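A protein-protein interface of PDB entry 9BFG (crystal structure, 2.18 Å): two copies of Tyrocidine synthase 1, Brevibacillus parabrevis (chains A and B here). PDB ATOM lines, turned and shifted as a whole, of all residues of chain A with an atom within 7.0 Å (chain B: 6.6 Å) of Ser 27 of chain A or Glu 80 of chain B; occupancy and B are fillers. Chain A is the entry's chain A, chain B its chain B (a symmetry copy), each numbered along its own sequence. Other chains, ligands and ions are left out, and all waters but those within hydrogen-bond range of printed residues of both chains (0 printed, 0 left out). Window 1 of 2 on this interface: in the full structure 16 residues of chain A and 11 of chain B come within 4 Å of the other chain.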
ATOM      1  N   THR A  21      29.920 -19.078 -10.772  1.00  0.00           N
ATOM      2  CA  THR A  21      30.848 -17.992 -11.155  1.00  0.00           C
ATOM      3  C   THR A  21      30.057 -16.712 -11.423  1.00  0.00           C
ATOM      4  O   THR A  21      30.456 -15.675 -10.865  1.00  0.00           O
ATOM      5  CB  THR A  21      31.719 -18.400 -12.338  1.00  0.00           C
ATOM      6  OG1 THR A  21      32.413 -19.544 -11.858  1.00  0.00           O
ATOM      7  CG2 THR A  21      32.698 -17.330 -12.777  1.00  0.00           C
ATOM      8  N   GLU A  22      28.984 -16.773 -12.216  1.00  0.00           N
ATOM      9  CA  GLU A  22      28.179 -15.567 -12.533  1.00  0.00           C
ATOM     10  C   GLU A  22      27.583 -14.968 -11.242  1.00  0.00           C
ATOM     11  O   GLU A  22      27.436 -13.755 -11.142  1.00  0.00           O
ATOM     12  CB  GLU A  22      27.060 -15.909 -13.519  1.00  0.00           C
ATOM     13  CG  GLU A  22      27.514 -16.060 -14.963  1.00  0.00           C
ATOM     14  CD  GLU A  22      26.469 -16.607 -15.930  1.00  0.00           C
ATOM     15  OE1 GLU A  22      25.276 -16.797 -15.544  1.00  0.00           O
ATOM     16  OE2 GLU A  22      26.845 -16.816 -17.079  1.00  0.00           O
ATOM     17  N   SER A  23      27.075 -15.816 -10.355  1.00  0.00           N
ATOM     18  CA  SER A  23      26.327 -15.375  -9.161  1.00  0.00           C
ATOM     19  C   SER A  23      27.348 -14.738  -8.200  1.00  0.00           C
ATOM     20  O   SER A  23      27.038 -13.702  -7.630  1.00  0.00           O
ATOM     21  CB  SER A  23      25.531 -16.525  -8.555  1.00  0.00           C
ATOM     22  OG  SER A  23      26.424 -17.504  -8.019  1.00  0.00           O
ATOM     23  N   ILE A  24      28.574 -15.265  -8.122  1.00  0.00           N
ATOM     24  CA  ILE A  24      29.681 -14.638  -7.346  1.00  0.00           C
ATOM     25  C   ILE A  24      30.079 -13.273  -7.948  1.00  0.00           C
ATOM     26  O   ILE A  24      30.142 -12.284  -7.193  1.00  0.00           O
ATOM     27  CB  ILE A  24      30.849 -15.618  -7.202  1.00  0.00           C
ATOM     28  CG1 ILE A  24      30.438 -16.795  -6.306  1.00  0.00           C
ATOM     29  CG2 ILE A  24      32.090 -14.907  -6.665  1.00  0.00           C
ATOM     30  CD1 ILE A  24      31.417 -17.962  -6.352  1.00  0.00           C
ATOM     31  N   LEU A  25      30.245 -13.189  -9.263  1.00  0.00           N
ATOM     32  CA  LEU A  25      30.478 -11.911  -9.978  1.00  0.00           C
ATOM     33  C   LEU A  25      29.339 -10.921  -9.738  1.00  0.00           C
ATOM     34  O   LEU A  25      29.661  -9.743  -9.490  1.00  0.00           O
ATOM     35  CB  LEU A  25      30.673 -12.181 -11.465  1.00  0.00           C
ATOM     36  CG  LEU A  25      32.034 -12.758 -11.834  1.00  0.00           C
ATOM     37  CD1 LEU A  25      32.004 -13.278 -13.263  1.00  0.00           C
ATOM     38  CD2 LEU A  25      33.148 -11.719 -11.652  1.00  0.00           C
ATOM     39  N   VAL A  26      28.069 -11.343  -9.798  1.00  0.00           N
ATOM     40  CA  VAL A  26      26.938 -10.412  -9.530  1.00  0.00           C
ATOM     41  C   VAL A  26      27.110  -9.836  -8.107  1.00  0.00           C
ATOM     42  O   VAL A  26      26.938  -8.638  -7.918  1.00  0.00           O
ATOM     43  CB  VAL A  26      25.564 -11.083  -9.745  1.00  0.00           C
ATOM     44  CG1 VAL A  26      24.422 -10.264  -9.166  1.00  0.00           C
ATOM     45  CG2 VAL A  26      25.298 -11.348 -11.230  1.00  0.00           C
ATOM     46  N   SER A  27      27.437 -10.680  -7.136  1.00  0.00           N
ATOM     47  CA  SER A  27      27.546 -10.307  -5.711  1.00  0.00           C
ATOM     48  C   SER A  27      28.709  -9.318  -5.559  1.00  0.00           C
ATOM     49  O   SER A  27      28.545  -8.233  -4.974  1.00  0.00           O
ATOM     50  CB  SER A  27      27.746 -11.536  -4.892  1.00  0.00           C
ATOM     51  OG  SER A  27      28.047 -11.201  -3.560  1.00  0.00           O
ATOM     52  N   ILE A  28      29.854  -9.663  -6.124  1.00  0.00           N
ATOM     53  CA  ILE A  28      31.031  -8.761  -6.107  1.00  0.00           C
ATOM     54  C   ILE A  28      30.664  -7.424  -6.771  1.00  0.00           C
ATOM     55  O   ILE A  28      30.954  -6.368  -6.180  1.00  0.00           O
ATOM     56  CB  ILE A  28      32.210  -9.454  -6.786  1.00  0.00           C
ATOM     57  CG1 ILE A  28      32.717 -10.601  -5.917  1.00  0.00           C
ATOM     58  CG2 ILE A  28      33.287  -8.430  -7.111  1.00  0.00           C
ATOM     59  CD1 ILE A  28      33.716 -11.473  -6.624  1.00  0.00           C
ATOM     60  N   TRP A  29      30.078  -7.443  -7.968  1.00  0.00           N
ATOM     61  CA  TRP A  29      29.780  -6.189  -8.704  1.00  0.00           C
ATOM     62  C   TRP A  29      28.795  -5.356  -7.889  1.00  0.00           C
ATOM     63  O   TRP A  29      28.958  -4.121  -7.859  1.00  0.00           O
ATOM     64  CB  TRP A  29      29.229  -6.429 -10.115  1.00  0.00           C
ATOM     65  CG  TRP A  29      30.206  -6.876 -11.162  1.00  0.00           C
ATOM     66  CD1 TRP A  29      31.331  -7.645 -11.014  1.00  0.00           C
ATOM     67  CD2 TRP A  29      30.099  -6.588 -12.556  1.00  0.00           C
ATOM     68  NE1 TRP A  29      31.937  -7.832 -12.226  1.00  0.00           N
ATOM     69  CE2 TRP A  29      31.190  -7.214 -13.195  1.00  0.00           C
ATOM     70  CE3 TRP A  29      29.187  -5.860 -13.328  1.00  0.00           C
ATOM     71  CZ2 TRP A  29      31.372  -7.146 -14.578  1.00  0.00           C
ATOM     72  CZ3 TRP A  29      29.377  -5.791 -14.693  1.00  0.00           C
ATOM     73  CH2 TRP A  29      30.451  -6.424 -15.304  1.00  0.00           C
ATOM     74  N   GLN A  30      27.781  -5.969  -7.273  1.00  0.00           N
ATOM     75  CA  GLN A  30      26.767  -5.175  -6.527  1.00  0.00           C
ATOM     76  C   GLN A  30      27.483  -4.429  -5.394  1.00  0.00           C
ATOM     77  O   GLN A  30      27.213  -3.253  -5.180  1.00  0.00           O
ATOM     78  CB  GLN A  30      25.634  -6.082  -6.048  1.00  0.00           C
ATOM     79  CG  GLN A  30      24.646  -6.394  -7.167  1.00  0.00           C
ATOM     80  CD  GLN A  30      23.553  -7.379  -6.845  1.00  0.00           C
ATOM     81  OE1 GLN A  30      22.697  -7.655  -7.685  1.00  0.00           O
ATOM     82  NE2 GLN A  30      23.600  -7.958  -5.654  1.00  0.00           N
ATOM     83  N   ASN A  31      28.386  -5.115  -4.713  1.00  0.00           N
ATOM     84  CA  ASN A  31      29.188  -4.572  -3.595  1.00  0.00           C
ATOM     85  C   ASN A  31      30.088  -3.426  -4.054  1.00  0.00           C
ATOM     86  O   ASN A  31      30.038  -2.363  -3.441  1.00  0.00           O
ATOM     87  CB  ASN A  31      30.082  -5.652  -2.998  1.00  0.00           C
ATOM     88  CG  ASN A  31      29.539  -6.086  -1.672  1.00  0.00           C
ATOM     89  OD1 ASN A  31      28.534  -6.790  -1.605  1.00  0.00           O
ATOM     90  ND2 ASN A  31      30.188  -5.619  -0.629  1.00  0.00           N
ATOM     91  N   VAL A  32      30.968  -3.694  -5.018  1.00  0.00           N
ATOM     92  CA  VAL A  32      31.991  -2.718  -5.475  1.00  0.00           C
ATOM     93  C   VAL A  32      31.276  -1.479  -6.037  1.00  0.00           C
ATOM     94  O   VAL A  32      31.651  -0.345  -5.717  1.00  0.00           O
ATOM     95  CB  VAL A  32      32.883  -3.398  -6.515  1.00  0.00           C
ATOM     96  CG1 VAL A  32      33.685  -2.387  -7.329  1.00  0.00           C
ATOM     97  CG2 VAL A  32      33.764  -4.420  -5.824  1.00  0.00           C
ATOM     98  N   ILE A  35      25.236  -0.796  -6.157  1.00  0.00           N
ATOM     99  CA  ILE A  35      24.037  -1.090  -6.987  1.00  0.00           C
ATOM    100  C   ILE A  35      23.373  -2.389  -6.542  1.00  0.00           C
ATOM    101  O   ILE A  35      24.072  -3.397  -6.409  1.00  0.00           O
ATOM    102  CB  ILE A  35      24.401  -1.090  -8.474  1.00  0.00           C
ATOM    103  CG1 ILE A  35      24.966   0.273  -8.869  1.00  0.00           C
ATOM    104  CG2 ILE A  35      23.195  -1.482  -9.312  1.00  0.00           C
ATOM    105  CD1 ILE A  35      25.457   0.347 -10.272  1.00  0.00           C
ATOM    106  N   ILE A  38      22.121  -6.143 -10.233  1.00  0.00           N
ATOM    107  CA  ILE A  38      22.928  -6.139 -11.476  1.00  0.00           C
ATOM    108  C   ILE A  38      22.557  -7.409 -12.222  1.00  0.00           C
ATOM    109  O   ILE A  38      22.603  -8.469 -11.603  1.00  0.00           O
ATOM    110  CB  ILE A  38      24.430  -6.056 -11.142  1.00  0.00           C
ATOM    111  CG1 ILE A  38      24.748  -4.686 -10.543  1.00  0.00           C
ATOM    112  CG2 ILE A  38      25.299  -6.370 -12.356  1.00  0.00           C
ATOM    113  CD1 ILE A  38      26.187  -4.493 -10.147  1.00  0.00           C
ATOM    114  N   ARG A  60      38.435  -8.961  -4.871  1.00  0.00           N
ATOM    115  CA  ARG A  60      37.381  -9.749  -4.186  1.00  0.00           C
ATOM    116  C   ARG A  60      37.327 -11.175  -4.759  1.00  0.00           C
ATOM    117  O   ARG A  60      37.122 -12.111  -3.976  1.00  0.00           O
ATOM    118  CB  ARG A  60      36.035  -9.047  -4.345  1.00  0.00           C
ATOM    119  CG  ARG A  60      35.890  -7.858  -3.412  1.00  0.00           C
ATOM    120  CD  ARG A  60      34.591  -7.132  -3.659  1.00  0.00           C
ATOM    121  NE  ARG A  60      34.471  -6.102  -2.642  1.00  0.00           N
ATOM    122  CZ  ARG A  60      33.915  -6.276  -1.468  1.00  0.00           C
ATOM    123  NH1 ARG A  60      33.915  -5.270  -0.621  1.00  0.00           N
ATOM    124  NH2 ARG A  60      33.380  -7.438  -1.129  1.00  0.00           N
ATOM    125  N   TYR A  64      37.805 -15.777  -3.454  1.00  0.00           N
ATOM    126  CA  TYR A  64      37.098 -17.036  -3.818  1.00  0.00           C
ATOM    127  C   TYR A  64      38.072 -17.979  -4.520  1.00  0.00           C
ATOM    128  O   TYR A  64      37.618 -18.966  -5.029  1.00  0.00           O
ATOM    129  CB  TYR A  64      35.890 -16.771  -4.724  1.00  0.00           C
ATOM    130  CG  TYR A  64      34.804 -15.960  -4.072  1.00  0.00           C
ATOM    131  CD1 TYR A  64      34.853 -14.572  -4.082  1.00  0.00           C
ATOM    132  CD2 TYR A  64      33.731 -16.582  -3.441  1.00  0.00           C
ATOM    133  CE1 TYR A  64      33.869 -13.813  -3.478  1.00  0.00           C
ATOM    134  CE2 TYR A  64      32.739 -15.835  -2.829  1.00  0.00           C
ATOM    135  CZ  TYR A  64      32.817 -14.452  -2.848  1.00  0.00           C
ATOM    136  OH  TYR A  64      31.876 -13.700  -2.226  1.00  0.00           O
ATOM    137  N   ILE A  79      29.096  -9.497 -17.017  1.00  0.00           N
ATOM    138  CA  ILE A  79      29.356 -10.722 -16.218  1.00  0.00           C
ATOM    139  C   ILE A  79      29.245 -11.932 -17.148  1.00  0.00           C
ATOM    140  O   ILE A  79      30.105 -12.834 -17.064  1.00  0.00           O
ATOM    141  CB  ILE A  79      28.386 -10.773 -15.022  1.00  0.00           C
ATOM    142  CG1 ILE A  79      28.750  -9.659 -14.023  1.00  0.00           C
ATOM    143  CG2 ILE A  79      28.388 -12.172 -14.422  1.00  0.00           C
ATOM    144  CD1 ILE A  79      27.739  -9.386 -12.932  1.00  0.00           C
ATOM    145  N   HIS B  15      32.031 -14.093   7.327  1.00  0.00           N
ATOM    146  CA  HIS B  15      31.611 -12.955   6.472  1.00  0.00           C
ATOM    147  C   HIS B  15      30.239 -12.477   6.926  1.00  0.00           C
ATOM    148  O   HIS B  15      29.238 -13.171   6.758  1.00  0.00           O
ATOM    149  CB  HIS B  15      31.662 -13.347   4.989  1.00  0.00           C
ATOM    150  CG  HIS B  15      32.994 -13.870   4.573  1.00  0.00           C
ATOM    151  ND1 HIS B  15      33.399 -15.173   4.841  1.00  0.00           N
ATOM    152  CD2 HIS B  15      34.024 -13.274   3.946  1.00  0.00           C
ATOM    153  CE1 HIS B  15      34.620 -15.358   4.368  1.00  0.00           C
ATOM    154  NE2 HIS B  15      35.023 -14.208   3.823  1.00  0.00           N
ATOM    155  N   ARG B  18      25.487  -7.929   4.648  1.00  0.00           N
ATOM    156  CA  ARG B  18      25.828  -6.630   4.011  1.00  0.00           C
ATOM    157  C   ARG B  18      24.539  -5.869   3.716  1.00  0.00           C
ATOM    158  O   ARG B  18      24.543  -4.645   3.900  1.00  0.00           O
ATOM    159  CB  ARG B  18      26.646  -6.851   2.734  1.00  0.00           C
ATOM    160  CG  ARG B  18      28.005  -7.493   2.966  1.00  0.00           C
ATOM    161  CD  ARG B  18      28.683  -7.902   1.678  1.00  0.00           C
ATOM    162  NE  ARG B  18      27.987  -8.982   0.974  1.00  0.00           N
ATOM    163  CZ  ARG B  18      28.590  -9.864   0.185  1.00  0.00           C
ATOM    164  NH1 ARG B  18      27.922 -10.846  -0.395  1.00  0.00           N
ATOM    165  NH2 ARG B  18      29.886  -9.775   0.005  1.00  0.00           N
ATOM    166  N   GLU B  22      20.289 -10.270   3.051  1.00  0.00           N
ATOM    167  CA  GLU B  22      21.378 -11.123   3.588  1.00  0.00           C
ATOM    168  C   GLU B  22      21.197 -11.311   5.107  1.00  0.00           C
ATOM    169  O   GLU B  22      21.591 -12.364   5.616  1.00  0.00           O
ATOM    170  CB  GLU B  22      22.747 -10.520   3.273  1.00  0.00           C
ATOM    171  CG  GLU B  22      23.203 -10.715   1.835  1.00  0.00           C
ATOM    172  CD  GLU B  22      24.650 -10.302   1.601  1.00  0.00           C
ATOM    173  OE1 GLU B  22      25.275  -9.747   2.536  1.00  0.00           O
ATOM    174  OE2 GLU B  22      25.169 -10.583   0.510  1.00  0.00           O
ATOM    175  N   LEU B  25      18.168 -13.581   5.975  1.00  0.00           N
ATOM    176  CA  LEU B  25      18.672 -14.946   5.668  1.00  0.00           C
ATOM    177  C   LEU B  25      19.633 -15.463   6.753  1.00  0.00           C
ATOM    178  O   LEU B  25      19.523 -16.655   7.096  1.00  0.00           O
ATOM    179  CB  LEU B  25      19.323 -14.944   4.286  1.00  0.00           C
ATOM    180  CG  LEU B  25      18.331 -14.952   3.126  1.00  0.00           C
ATOM    181  CD1 LEU B  25      19.010 -14.523   1.843  1.00  0.00           C
ATOM    182  CD2 LEU B  25      17.691 -16.329   2.950  1.00  0.00           C
ATOM    183  N   TRP B  29      18.556 -18.793   8.721  1.00  0.00           N
ATOM    184  CA  TRP B  29      19.418 -20.004   8.677  1.00  0.00           C
ATOM    185  C   TRP B  29      19.782 -20.393  10.111  1.00  0.00           C
ATOM    186  O   TRP B  29      19.854 -21.590  10.396  1.00  0.00           O
ATOM    187  CB  TRP B  29      20.680 -19.807   7.820  1.00  0.00           C
ATOM    188  CG  TRP B  29      20.441 -19.834   6.341  1.00  0.00           C
ATOM    189  CD1 TRP B  29      19.303 -19.448   5.694  1.00  0.00           C
ATOM    190  CD2 TRP B  29      21.356 -20.262   5.317  1.00  0.00           C
ATOM    191  NE1 TRP B  29      19.452 -19.597   4.342  1.00  0.00           N
ATOM    192  CE2 TRP B  29      20.696 -20.110   4.080  1.00  0.00           C
ATOM    193  CE3 TRP B  29      22.675 -20.741   5.315  1.00  0.00           C
ATOM    194  CZ2 TRP B  29      21.306 -20.416   2.856  1.00  0.00           C
ATOM    195  CZ3 TRP B  29      23.277 -21.061   4.115  1.00  0.00           C
ATOM    196  CH2 TRP B  29      22.602 -20.888   2.894  1.00  0.00           C
ATOM    197  N   GLY B  39      27.841 -17.199   8.678  1.00  0.00           N
ATOM    198  CA  GLY B  39      28.369 -16.284   7.650  1.00  0.00           C
ATOM    199  C   GLY B  39      27.716 -16.498   6.300  1.00  0.00           C
ATOM    200  O   GLY B  39      27.259 -17.639   6.026  1.00  0.00           O
ATOM    201  N   ILE B  40      27.769 -15.462   5.456  1.00  0.00           N
ATOM    202  CA  ILE B  40      27.103 -15.408   4.121  1.00  0.00           C
ATOM    203  C   ILE B  40      27.838 -16.278   3.093  1.00  0.00           C
ATOM    204  O   ILE B  40      27.340 -16.393   1.954  1.00  0.00           O
ATOM    205  CB  ILE B  40      26.973 -13.956   3.660  1.00  0.00           C
ATOM    206  CG1 ILE B  40      28.348 -13.361   3.307  1.00  0.00           C
ATOM    207  CG2 ILE B  40      26.207 -13.172   4.717  1.00  0.00           C
ATOM    208  CD1 ILE B  40      28.300 -11.980   2.700  1.00  0.00           C
ATOM    209  N   ARG B  41      28.962 -16.888   3.453  1.00  0.00           N
ATOM    210  CA  ARG B  41      29.632 -17.846   2.555  1.00  0.00           C
ATOM    211  C   ARG B  41      29.528 -19.254   3.105  1.00  0.00           C
ATOM    212  O   ARG B  41      30.073 -20.132   2.442  1.00  0.00           O
ATOM    213  CB  ARG B  41      31.103 -17.514   2.378  1.00  0.00           C
ATOM    214  CG  ARG B  41      31.346 -16.245   1.591  1.00  0.00           C
ATOM    215  CD  ARG B  41      32.754 -16.333   1.027  1.00  0.00           C
ATOM    216  NE  ARG B  41      33.205 -15.001   0.682  1.00  0.00           N
ATOM    217  CZ  ARG B  41      34.405 -14.705   0.179  1.00  0.00           C
ATOM    218  NH1 ARG B  41      34.690 -13.447  -0.081  1.00  0.00           N
ATOM    219  NH2 ARG B  41      35.313 -15.644  -0.053  1.00  0.00           N
ATOM    220  N   TYR B  76      22.181 -22.669  -5.182  1.00  0.00           N
ATOM    221  CA  TYR B  76      22.985 -21.475  -4.814  1.00  0.00           C
ATOM    222  C   TYR B  76      23.154 -21.458  -3.291  1.00  0.00           C
ATOM    223  O   TYR B  76      22.637 -20.577  -2.611  1.00  0.00           O
ATOM    224  CB  TYR B  76      22.345 -20.221  -5.435  1.00  0.00           C
ATOM    225  CG  TYR B  76      22.291 -20.243  -6.945  1.00  0.00           C
ATOM    226  CD1 TYR B  76      23.438 -20.075  -7.699  1.00  0.00           C
ATOM    227  CD2 TYR B  76      21.108 -20.515  -7.624  1.00  0.00           C
ATOM    228  CE1 TYR B  76      23.408 -20.147  -9.080  1.00  0.00           C
ATOM    229  CE2 TYR B  76      21.056 -20.585  -9.006  1.00  0.00           C
ATOM    230  CZ  TYR B  76      22.211 -20.390  -9.739  1.00  0.00           C
ATOM    231  OH  TYR B  76      22.187 -20.481 -11.105  1.00  0.00           O
ATOM    232  N   THR B  78      24.686 -20.629  -0.553  1.00  0.00           N
ATOM    233  CA  THR B  78      25.263 -19.661   0.406  1.00  0.00           C
ATOM    234  C   THR B  78      24.321 -18.472   0.432  1.00  0.00           C
ATOM    235  O   THR B  78      23.596 -18.262  -0.540  1.00  0.00           O
ATOM    236  CB  THR B  78      26.698 -19.225   0.055  1.00  0.00           C
ATOM    237  OG1 THR B  78      26.687 -18.345  -1.077  1.00  0.00           O
ATOM    238  CG2 THR B  78      27.636 -20.382  -0.200  1.00  0.00           C
ATOM    239  N   ILE B  79      24.337 -17.733   1.514  1.00  0.00           N
ATOM    240  CA  ILE B  79      23.357 -16.651   1.727  1.00  0.00           C
ATOM    241  C   ILE B  79      23.615 -15.541   0.720  1.00  0.00           C
ATOM    242  O   ILE B  79      22.624 -14.920   0.300  1.00  0.00           O
ATOM    243  CB  ILE B  79      23.415 -16.176   3.174  1.00  0.00           C
ATOM    244  CG1 ILE B  79      22.756 -17.221   4.078  1.00  0.00           C
ATOM    245  CG2 ILE B  79      22.776 -14.811   3.320  1.00  0.00           C
ATOM    246  CD1 ILE B  79      22.953 -16.989   5.560  1.00  0.00           C
ATOM    247  N   GLU B  80      24.877 -15.271   0.383  1.00  0.00           N
ATOM    248  CA  GLU B  80      25.207 -14.156  -0.553  1.00  0.00           C
ATOM    249  C   GLU B  80      24.658 -14.522  -1.937  1.00  0.00           C
ATOM    250  O   GLU B  80      24.061 -13.649  -2.570  1.00  0.00           O
ATOM    251  CB  GLU B  80      26.696 -13.796  -0.564  1.00  0.00           C
ATOM    252  CG  GLU B  80      27.655 -14.867  -1.060  1.00  0.00           C
ATOM    253  CD  GLU B  80      29.092 -14.341  -1.171  1.00  0.00           C
ATOM    254  OE1 GLU B  80      29.272 -13.111  -0.995  1.00  0.00           O
ATOM    255  OE2 GLU B  80      30.030 -15.148  -1.442  1.00  0.00           O
ATOM    256  N   GLN B  81      24.766 -15.785  -2.344  1.00  0.00           N
ATOM    257  CA  GLN B  81      24.228 -16.255  -3.640  1.00  0.00           C
ATOM    258  C   GLN B  81      22.705 -16.271  -3.629  1.00  0.00           C
ATOM    259  O   GLN B  81      22.115 -15.764  -4.591  1.00  0.00           O
ATOM    260  CB  GLN B  81      24.789 -17.626  -3.962  1.00  0.00           C
ATOM    261  CG  GLN B  81      26.273 -17.558  -4.239  1.00  0.00           C
ATOM    262  CD  GLN B  81      26.798 -18.947  -4.422  1.00  0.00           C
ATOM    263  OE1 GLN B  81      27.210 -19.586  -3.460  1.00  0.00           O
ATOM    264  NE2 GLN B  81      26.690 -19.452  -5.637  1.00  0.00           N
ATOM    265  N   VAL B  82      22.085 -16.830  -2.592  1.00  0.00           N
ATOM    266  CA  VAL B  82      20.622 -17.105  -2.588  1.00  0.00           C
ATOM    267  C   VAL B  82      19.876 -15.771  -2.482  1.00  0.00           C
ATOM    268  O   VAL B  82      18.799 -15.650  -3.113  1.00  0.00           O
ATOM    269  CB  VAL B  82      20.182 -18.104  -1.494  1.00  0.00           C
ATOM    270  CG1 VAL B  82      20.050 -17.470  -0.142  1.00  0.00           C
ATOM    271  CG2 VAL B  82      18.840 -18.727  -1.850  1.00  0.00           C
ATOM    272  N   ALA B  83      20.414 -14.802  -1.746  1.00  0.00           N
ATOM    273  CA  ALA B  83      19.858 -13.425  -1.660  1.00  0.00           C
ATOM    274  C   ALA B  83      19.584 -12.854  -3.071  1.00  0.00           C
ATOM    275  O   ALA B  83      18.585 -12.155  -3.209  1.00  0.00           O
ATOM    276  CB  ALA B  83      20.776 -12.527  -0.870  1.00  0.00           C
ATOM    277  N   LEU B  84      20.381 -13.214  -4.091  1.00  0.00           N
ATOM    278  CA  LEU B  84      20.215 -12.678  -5.471  1.00  0.00           C
ATOM    279  C   LEU B  84      18.897 -13.193  -6.073  1.00  0.00           C
ATOM    280  O   LEU B  84      18.376 -12.513  -6.956  1.00  0.00           O
ATOM    281  CB  LEU B  84      21.407 -13.077  -6.345  1.00  0.00           C
ATOM    282  CG  LEU B  84      22.795 -12.764  -5.800  1.00  0.00           C
ATOM    283  CD1 LEU B  84      23.859 -13.355  -6.700  1.00  0.00           C
ATOM    284  CD2 LEU B  84      22.995 -11.270  -5.614  1.00  0.00           C
ATOM    285  N   PHE B  85      18.349 -14.321  -5.587  1.00  0.00           N
ATOM    286  CA  PHE B  85      17.113 -14.940  -6.119  1.00  0.00           C
ATOM    287  C   PHE B  85      15.922 -14.655  -5.208  1.00  0.00           C
ATOM    288  O   PHE B  85      14.832 -15.069  -5.564  1.00  0.00           O
ATOM    289  CB  PHE B  85      17.321 -16.440  -6.301  1.00  0.00           C
ATOM    290  CG  PHE B  85      18.458 -16.732  -7.237  1.00  0.00           C
ATOM    291  CD1 PHE B  85      18.256 -16.730  -8.604  1.00  0.00           C
ATOM    292  CD2 PHE B  85      19.736 -16.940  -6.748  1.00  0.00           C
ATOM    293  CE1 PHE B  85      19.307 -16.971  -9.472  1.00  0.00           C
ATOM    294  CE2 PHE B  85      20.790 -17.151  -7.617  1.00  0.00           C
ATOM    295  CZ  PHE B  85      20.568 -17.183  -8.974  1.00  0.00           C
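OH of Tyr 64 of chain A is in hydrogen-bond range of NE of Arg 41 of chain B.
OE1 of Glu 80 of chain B is in hydrogen-bond range of OG of Ser 27 of chain A, at 3.4 Å.
The side-chain hydroxyl (OG) of Ser 27 of chain A is in hydrogen-bond range of the guanidinium group (NH1) of Arg 18 of chain B, 3.2 Å away.
The side-chain hydroxyl (OG) of Ser 23 of chain A lies within hydrogen-bond range of the side-chain amide nitrogen (NE2) of Gln 81 of chain B.
OD1 of Asn 31 of chain A sits at hydrogen-bond distance from NE of Arg 18 of chain B (3.4 Å).
OE2 of Glu 80 of chain B is in hydrogen-bond range of OH of Tyr 64 of chain A (2.5 Å).
Positions printed for both chains: 22, 25, 29 and 79.
Of the 10 pairs that touch across the chains among the printed residues, none has its exchanged pair printed and touching as well.
The guanidinium group of Arg 41 of chain B is in salt-bridge range of the side-chain carboxylate of Glu 80 of chain B, at 3.8 Å.
The side-chain carboxylate (OE1) of Glu 80 of chain B lies within salt-bridge range of the guanidinium group (NH1) of Arg 18 of chain B (2.7 Å).
OE1 of Gln 30 of chain A sits at hydrogen-bond distance from N of Ile 38 of chain A (3.0 Å).
The backbone NH (N) of Ile 35 of chain A lies within hydrogen-bond range of the backbone carbonyl oxygen (O) of Gln 30 of chain A (3.3 Å).
The backbone carbonyl oxygen of Ile 40 of chain B is in hydrogen-bond range of the backbone NH of Glu 80 of chain B, at 3.1 Å.
NH1 of Arg 18 of chain B is in salt-bridge range of OE2 of Glu 22 of chain B (2.9 Å).
Ser 27 of chain A touches two residues of chain B.
Of chain A, only Ser 27 (3.4 Å) and Tyr 64 (2.5 Å) come within 4 Å of Glu 80 of chain B.
Printed residues of chain A within 4 Å of Arg 18 of chain B: Ser 27 and Asn 31.
Of the printed residues of chain B, Tyr 64 of chain A touches Arg 41 (3.4 Å) and Glu 80 (2.5 Å).
Of the printed residues of chain A, Tyr 76 of chain B touches Ser 23.
Of the printed residues of chain B, Ser 23 of chain A touches Tyr 76, Gln 81 and Leu 84.
Printed residues of chain B within 4 Å of Asn 31 of chain A: Arg 18.
Arg 60 of chain A touches none of the printed residues of chain B.
The nearest residue of chain B that does not touch Ser 27 of chain A is Leu 84 of chain B (4.5 Å).
The nearest printed residue of chain A that does not touch Arg 41 of chain B is Arg 60 of chain A (4.8 Å).
OG of Ser 23 of chain A touches CD1 of Tyr 76 of chain B, 3.95 Å away.
Leu 84 of chain B touches Ser 23 of chain A.
Leu 84 of chain B touches Val 26 of chain A (CD2 to CG1, 3.96 Å).
CD2 of Leu 84 of chain B touches NE2 of Gln 30 of chain A, 3.4 Å away.
Hydrophobic or aromatic side chains of chain B that line the printed part of chain A: Tyr 76 and Leu 84.
Of the 17 printed residues of chain A, 6 touch a printed residue of chain B.
Hydrophobic or aromatic side chains of chain A that line the printed part of chain B: Val 26 and Tyr 64.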
